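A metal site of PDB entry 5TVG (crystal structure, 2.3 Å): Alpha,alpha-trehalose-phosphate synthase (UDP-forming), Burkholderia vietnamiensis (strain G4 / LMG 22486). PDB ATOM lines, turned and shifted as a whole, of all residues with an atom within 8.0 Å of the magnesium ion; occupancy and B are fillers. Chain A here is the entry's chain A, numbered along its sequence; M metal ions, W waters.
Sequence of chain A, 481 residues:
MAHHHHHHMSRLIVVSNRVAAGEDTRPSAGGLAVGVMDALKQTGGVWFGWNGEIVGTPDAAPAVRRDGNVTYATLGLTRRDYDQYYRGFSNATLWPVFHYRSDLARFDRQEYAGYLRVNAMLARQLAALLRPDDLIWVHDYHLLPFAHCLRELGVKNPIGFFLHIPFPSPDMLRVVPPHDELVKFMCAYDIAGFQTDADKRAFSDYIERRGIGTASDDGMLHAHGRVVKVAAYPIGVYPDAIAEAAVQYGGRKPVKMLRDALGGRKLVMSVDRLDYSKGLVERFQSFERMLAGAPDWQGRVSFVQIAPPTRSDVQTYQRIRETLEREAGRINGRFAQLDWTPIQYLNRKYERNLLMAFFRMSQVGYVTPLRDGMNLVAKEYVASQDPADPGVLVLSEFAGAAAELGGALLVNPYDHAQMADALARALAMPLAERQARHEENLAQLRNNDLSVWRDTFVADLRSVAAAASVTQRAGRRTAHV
The guanidinium group (NH2) of Arg 360 lies within salt-bridge range of the side-chain carboxylate (OD2) of Asp 386 (3.98 Å).
The backbone carbonyl oxygen of Ser 384 lies within hydrogen-bond range of the guanidinium group of Arg 360 (2.8 Å).
The backbone carbonyl oxygen of Phe 359 lies within hydrogen-bond range of the side-chain amide nitrogen of Gln 385 (2.7 Å).
The side-chain amide oxygen (OE1) of Gln 385 lies close to the backbone NH (N) of Gly 391.
The backbone carbonyl oxygen of Tyr 381 lies within hydrogen-bond range of the side-chain amide nitrogen of Gln 385.
O of Phe 359 is in hydrogen-bond range of OG of Ser 362 (2.6 Å).
OH of Tyr 381 sits at hydrogen-bond distance from OG of Ser 362 (3.0 Å).
The backbone carbonyl oxygen of Met 361 sits at hydrogen-bond distance from the side-chain amide nitrogen of Gln 363 (3.2 Å).
Residues that only touch the magnesium ion: Phe 359 (3.5 Å), Met 361 (3.9 Å) and Gly 391 (3.8 Å).
Along chain A the residues within 4 Å of the magnesium ion span positions 359 to 391.
The magnesium ion is bound by the backbone carbonyl oxygen (O) of Arg 360 (2.1 Å), the side-chain amide oxygen (OE1) of Gln 385 (2.2 Å), the backbone carbonyl oxygen (O) of Ser 362 (2.3 Å) and water W2 (2.6 Å).
The magnesium ion has four donor atoms within binding distance.
Slightly farther from the magnesium ion lies water W1 (2.7 Å).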
ATOM      1  N   LEU A 267     -11.898 -25.643  13.637  1.00  0.00           N
ATOM      2  CA  LEU A 267     -10.923 -26.220  14.557  1.00  0.00           C
ATOM      3  C   LEU A 267     -11.591 -27.339  15.340  1.00  0.00           C
ATOM      4  O   LEU A 267     -12.596 -27.115  16.010  1.00  0.00           O
ATOM      5  CB  LEU A 267     -10.373 -25.136  15.485  1.00  0.00           C
ATOM      6  CG  LEU A 267      -9.535 -25.638  16.678  1.00  0.00           C
ATOM      7  CD1 LEU A 267      -8.244 -26.365  16.162  1.00  0.00           C
ATOM      8  CD2 LEU A 267      -9.233 -24.519  17.632  1.00  0.00           C
ATOM      9  N   MET A 356      -8.304 -23.749  28.117  1.00  0.00           N
ATOM     10  CA  MET A 356      -9.686 -23.256  28.077  1.00  0.00           C
ATOM     11  C   MET A 356      -9.898 -22.271  26.929  1.00  0.00           C
ATOM     12  O   MET A 356     -10.939 -22.307  26.261  1.00  0.00           O
ATOM     13  CB  MET A 356     -10.049 -22.609  29.419  1.00  0.00           C
ATOM     14  CG  MET A 356      -9.707 -23.526  30.619  1.00  0.00           C
ATOM     15  SD  MET A 356     -10.440 -25.178  30.460  1.00  0.00           S
ATOM     16  CE  MET A 356      -9.415 -26.151  31.529  1.00  0.00           C
ATOM     17  N   ALA A 357      -8.934 -21.386  26.682  1.00  0.00           N
ATOM     18  CA  ALA A 357      -9.079 -20.497  25.529  1.00  0.00           C
ATOM     19  C   ALA A 357      -9.048 -21.265  24.204  1.00  0.00           C
ATOM     20  O   ALA A 357      -9.688 -20.827  23.234  1.00  0.00           O
ATOM     21  CB  ALA A 357      -8.000 -19.404  25.566  1.00  0.00           C
ATOM     22  N   PHE A 358      -8.299 -22.380  24.114  1.00  0.00           N
ATOM     23  CA  PHE A 358      -8.312 -23.226  22.904  1.00  0.00           C
ATOM     24  C   PHE A 358      -9.685 -23.870  22.697  1.00  0.00           C
ATOM     25  O   PHE A 358     -10.205 -23.879  21.578  1.00  0.00           O
ATOM     26  CB  PHE A 358      -7.243 -24.332  22.983  1.00  0.00           C
ATOM     27  CG  PHE A 358      -5.829 -23.836  23.094  1.00  0.00           C
ATOM     28  CD1 PHE A 358      -5.462 -22.586  22.622  1.00  0.00           C
ATOM     29  CD2 PHE A 358      -4.857 -24.625  23.699  1.00  0.00           C
ATOM     30  CE1 PHE A 358      -4.154 -22.123  22.745  1.00  0.00           C
ATOM     31  CE2 PHE A 358      -3.553 -24.186  23.849  1.00  0.00           C
ATOM     32  CZ  PHE A 358      -3.194 -22.918  23.362  1.00  0.00           C
ATOM     33  N   PHE A 359     -10.262 -24.451  23.767  1.00  0.00           N
ATOM     34  CA  PHE A 359     -11.593 -25.064  23.697  1.00  0.00           C
ATOM     35  C   PHE A 359     -12.627 -24.057  23.199  1.00  0.00           C
ATOM     36  O   PHE A 359     -13.441 -24.383  22.326  1.00  0.00           O
ATOM     37  CB  PHE A 359     -12.016 -25.582  25.079  1.00  0.00           C
ATOM     38  CG  PHE A 359     -11.199 -26.758  25.564  1.00  0.00           C
ATOM     39  CD1 PHE A 359     -10.529 -27.580  24.669  1.00  0.00           C
ATOM     40  CD2 PHE A 359     -11.042 -26.977  26.949  1.00  0.00           C
ATOM     41  CE1 PHE A 359      -9.766 -28.650  25.126  1.00  0.00           C
ATOM     42  CE2 PHE A 359     -10.299 -28.042  27.415  1.00  0.00           C
ATOM     43  CZ  PHE A 359      -9.652 -28.887  26.496  1.00  0.00           C
ATOM     44  N   ARG A 360     -12.625 -22.847  23.749  1.00  0.00           N
ATOM     45  CA  ARG A 360     -13.598 -21.828  23.330  1.00  0.00           C
ATOM     46  C   ARG A 360     -13.462 -21.492  21.847  1.00  0.00           C
ATOM     47  O   ARG A 360     -14.471 -21.320  21.152  1.00  0.00           O
ATOM     48  CB  ARG A 360     -13.395 -20.579  24.168  1.00  0.00           C
ATOM     49  CG  ARG A 360     -14.423 -19.483  23.998  1.00  0.00           C
ATOM     50  CD  ARG A 360     -14.176 -18.439  25.108  1.00  0.00           C
ATOM     51  NE  ARG A 360     -15.200 -17.407  25.163  1.00  0.00           N
ATOM     52  CZ  ARG A 360     -16.234 -17.431  25.985  1.00  0.00           C
ATOM     53  NH1 ARG A 360     -16.404 -18.449  26.836  1.00  0.00           N
ATOM     54  NH2 ARG A 360     -17.119 -16.434  25.954  1.00  0.00           N
ATOM     55  N   MET A 361     -12.237 -21.352  21.364  1.00  0.00           N
ATOM     56  CA  MET A 361     -12.008 -20.986  19.965  1.00  0.00           C
ATOM     57  C   MET A 361     -12.527 -22.068  19.025  1.00  0.00           C
ATOM     58  O   MET A 361     -12.990 -21.754  17.930  1.00  0.00           O
ATOM     59  CB  MET A 361     -10.515 -20.711  19.700  1.00  0.00           C
ATOM     60  CG  MET A 361     -10.196 -20.138  18.305  1.00  0.00           C
ATOM     61  SD  MET A 361      -8.384 -20.178  17.986  1.00  0.00           S
ATOM     62  CE  MET A 361      -7.852 -20.126  19.685  1.00  0.00           C
ATOM     63  N   SER A 362     -12.470 -23.333  19.452  1.00  0.00           N
ATOM     64  CA  SER A 362     -12.795 -24.456  18.583  1.00  0.00           C
ATOM     65  C   SER A 362     -14.292 -24.573  18.317  1.00  0.00           C
ATOM     66  O   SER A 362     -15.132 -24.044  19.046  1.00  0.00           O
ATOM     67  CB  SER A 362     -12.325 -25.774  19.195  1.00  0.00           C
ATOM     68  OG  SER A 362     -13.037 -26.014  20.402  1.00  0.00           O
ATOM     69  N   GLN A 363     -14.597 -25.317  17.239  1.00  0.00           N
ATOM     70  CA  GLN A 363     -15.975 -25.671  16.902  1.00  0.00           C
ATOM     71  C   GLN A 363     -16.359 -27.035  17.447  1.00  0.00           C
ATOM     72  O   GLN A 363     -17.544 -27.288  17.659  1.00  0.00           O
ATOM     73  CB  GLN A 363     -16.161 -25.679  15.362  1.00  0.00           C
ATOM     74  CG  GLN A 363     -16.224 -24.276  14.751  1.00  0.00           C
ATOM     75  CD  GLN A 363     -14.913 -23.437  14.947  1.00  0.00           C
ATOM     76  OE1 GLN A 363     -13.821 -23.845  14.564  1.00  0.00           O
ATOM     77  NE2 GLN A 363     -15.055 -22.296  15.581  1.00  0.00           N
ATOM     78  N   VAL A 364     -15.393 -27.924  17.685  1.00  0.00           N
ATOM     79  CA  VAL A 364     -15.683 -29.282  18.113  1.00  0.00           C
ATOM     80  C   VAL A 364     -14.717 -29.682  19.213  1.00  0.00           C
ATOM     81  O   VAL A 364     -13.502 -29.480  19.097  1.00  0.00           O
ATOM     82  CB  VAL A 364     -15.549 -30.286  16.944  1.00  0.00           C
ATOM     83  CG1 VAL A 364     -15.838 -31.704  17.420  1.00  0.00           C
ATOM     84  CG2 VAL A 364     -16.442 -29.886  15.770  1.00  0.00           C
ATOM     85  N   GLY A 365     -15.259 -30.313  20.275  1.00  0.00           N
ATOM     86  CA  GLY A 365     -14.436 -31.020  21.244  1.00  0.00           C
ATOM     87  C   GLY A 365     -14.537 -32.514  20.980  1.00  0.00           C
ATOM     88  O   GLY A 365     -15.621 -33.084  20.977  1.00  0.00           O
ATOM     89  N   TYR A 381     -14.426 -28.654  28.383  1.00  0.00           N
ATOM     90  CA  TYR A 381     -14.707 -28.176  27.033  1.00  0.00           C
ATOM     91  C   TYR A 381     -16.047 -27.458  26.993  1.00  0.00           C
ATOM     92  O   TYR A 381     -16.167 -26.374  26.408  1.00  0.00           O
ATOM     93  CB  TYR A 381     -14.682 -29.351  26.017  1.00  0.00           C
ATOM     94  CG  TYR A 381     -14.950 -28.857  24.621  1.00  0.00           C
ATOM     95  CD1 TYR A 381     -13.930 -28.374  23.820  1.00  0.00           C
ATOM     96  CD2 TYR A 381     -16.252 -28.784  24.124  1.00  0.00           C
ATOM     97  CE1 TYR A 381     -14.169 -27.874  22.536  1.00  0.00           C
ATOM     98  CE2 TYR A 381     -16.512 -28.288  22.852  1.00  0.00           C
ATOM     99  CZ  TYR A 381     -15.475 -27.825  22.066  1.00  0.00           C
ATOM    100  OH  TYR A 381     -15.744 -27.317  20.791  1.00  0.00           O
ATOM    101  N   VAL A 382     -17.091 -28.074  27.561  1.00  0.00           N
ATOM    102  CA  VAL A 382     -18.411 -27.420  27.569  1.00  0.00           C
ATOM    103  C   VAL A 382     -18.321 -26.069  28.256  1.00  0.00           C
ATOM    104  O   VAL A 382     -18.775 -25.046  27.724  1.00  0.00           O
ATOM    105  CB  VAL A 382     -19.469 -28.321  28.237  1.00  0.00           C
ATOM    106  CG1 VAL A 382     -20.746 -27.539  28.540  1.00  0.00           C
ATOM    107  CG2 VAL A 382     -19.721 -29.571  27.369  1.00  0.00           C
ATOM    108  N   SER A 384     -15.989 -23.954  28.626  1.00  0.00           N
ATOM    109  CA  SER A 384     -15.213 -22.902  28.004  1.00  0.00           C
ATOM    110  C   SER A 384     -15.989 -22.164  26.944  1.00  0.00           C
ATOM    111  O   SER A 384     -15.557 -21.082  26.506  1.00  0.00           O
ATOM    112  CB  SER A 384     -13.938 -23.486  27.356  1.00  0.00           C
ATOM    113  OG  SER A 384     -13.104 -24.122  28.326  1.00  0.00           O
ATOM    114  N   GLN A 385     -17.112 -22.727  26.483  1.00  0.00           N
ATOM    115  CA  GLN A 385     -17.725 -22.212  25.273  1.00  0.00           C
ATOM    116  C   GLN A 385     -18.416 -20.887  25.513  1.00  0.00           C
ATOM    117  O   GLN A 385     -18.960 -20.622  26.589  1.00  0.00           O
ATOM    118  CB  GLN A 385     -18.726 -23.214  24.661  1.00  0.00           C
ATOM    119  CG  GLN A 385     -18.112 -24.549  24.228  1.00  0.00           C
ATOM    120  CD  GLN A 385     -16.939 -24.359  23.287  1.00  0.00           C
ATOM    121  OE1 GLN A 385     -17.095 -23.811  22.186  1.00  0.00           O
ATOM    122  NE2 GLN A 385     -15.747 -24.780  23.715  1.00  0.00           N
ATOM    123  N   ASP A 386     -18.454 -20.075  24.482  1.00  0.00           N
ATOM    124  CA  ASP A 386     -19.293 -18.903  24.465  1.00  0.00           C
ATOM    125  C   ASP A 386     -20.739 -19.298  24.171  1.00  0.00           C
ATOM    126  O   ASP A 386     -21.007 -19.858  23.094  1.00  0.00           O
ATOM    127  CB  ASP A 386     -18.764 -17.944  23.407  1.00  0.00           C
ATOM    128  CG  ASP A 386     -19.544 -16.659  23.337  1.00  0.00           C
ATOM    129  OD1 ASP A 386     -20.592 -16.520  24.020  1.00  0.00           O
ATOM    130  OD2 ASP A 386     -19.105 -15.784  22.572  1.00  0.00           O
ATOM    131  N   ASP A 389     -22.205 -18.617  20.772  1.00  0.00           N
ATOM    132  CA  ASP A 389     -21.713 -19.385  19.627  1.00  0.00           C
ATOM    133  C   ASP A 389     -20.933 -20.602  20.134  1.00  0.00           C
ATOM    134  O   ASP A 389     -19.692 -20.623  20.100  1.00  0.00           O
ATOM    135  CB  ASP A 389     -20.845 -18.505  18.740  1.00  0.00           C
ATOM    136  CG  ASP A 389     -20.476 -19.170  17.444  1.00  0.00           C
ATOM    137  OD1 ASP A 389     -20.977 -20.289  17.177  1.00  0.00           O
ATOM    138  OD2 ASP A 389     -19.610 -18.616  16.740  1.00  0.00           O
ATOM    139  N   PRO A 390     -21.609 -21.609  20.669  1.00  0.00           N
ATOM    140  CA  PRO A 390     -20.906 -22.706  21.342  1.00  0.00           C
ATOM    141  C   PRO A 390     -20.546 -23.855  20.417  1.00  0.00           C
ATOM    142  O   PRO A 390     -21.224 -24.162  19.423  1.00  0.00           O
ATOM    143  CB  PRO A 390     -21.916 -23.145  22.421  1.00  0.00           C
ATOM    144  CG  PRO A 390     -23.286 -22.874  21.767  1.00  0.00           C
ATOM    145  CD  PRO A 390     -23.079 -21.679  20.856  1.00  0.00           C
ATOM    146  N   GLY A 391     -19.388 -24.459  20.730  1.00  0.00           N
ATOM    147  CA  GLY A 391     -18.934 -25.621  20.003  1.00  0.00           C
ATOM    148  C   GLY A 391     -19.683 -26.867  20.429  1.00  0.00           C
ATOM    149  O   GLY A 391     -20.416 -26.881  21.418  1.00  0.00           O
ATOM    150  N   VAL A 392     -19.401 -27.966  19.719  1.00  0.00           N
ATOM    151  CA  VAL A 392     -20.105 -29.222  19.908  1.00  0.00           C
ATOM    152  C   VAL A 392     -19.177 -30.237  20.544  1.00  0.00           C
ATOM    153  O   VAL A 392     -18.041 -30.418  20.099  1.00  0.00           O
ATOM    154  CB  VAL A 392     -20.639 -29.776  18.554  1.00  0.00           C
ATOM    155  CG1 VAL A 392     -21.287 -31.133  18.749  1.00  0.00           C
ATOM    156  CG2 VAL A 392     -21.595 -28.808  17.962  1.00  0.00           C
ATOM    157  N   ARG A 434     -26.906 -26.190  18.501  1.00  0.00           N
ATOM    158  CA  ARG A 434     -25.683 -26.126  19.294  1.00  0.00           C
ATOM    159  C   ARG A 434     -25.951 -25.453  20.638  1.00  0.00           C
ATOM    160  O   ARG A 434     -25.433 -25.886  21.671  1.00  0.00           O
ATOM    161  CB  ARG A 434     -24.584 -25.370  18.541  1.00  0.00           C
ATOM    162  CG  ARG A 434     -24.058 -26.126  17.308  1.00  0.00           C
ATOM    163  CD  ARG A 434     -22.792 -25.520  16.708  1.00  0.00           C
ATOM    164  NE  ARG A 434     -23.070 -24.385  15.842  1.00  0.00           N
ATOM    165  CZ  ARG A 434     -22.768 -23.109  16.110  1.00  0.00           C
ATOM    166  NH1 ARG A 434     -22.173 -22.784  17.277  1.00  0.00           N
ATOM    167  NH2 ARG A 434     -23.084 -22.163  15.224  1.00  0.00           N
HETATM  168 MG    MG M   1     -15.991 -22.675  20.645  1.00  0.00          MG
HETATM  169  O   HOH W   1     -17.306 -20.575  21.636  1.00  0.00           O
HETATM  170  O   HOH W   2     -17.723 -22.094  18.864  1.00  0.00           O
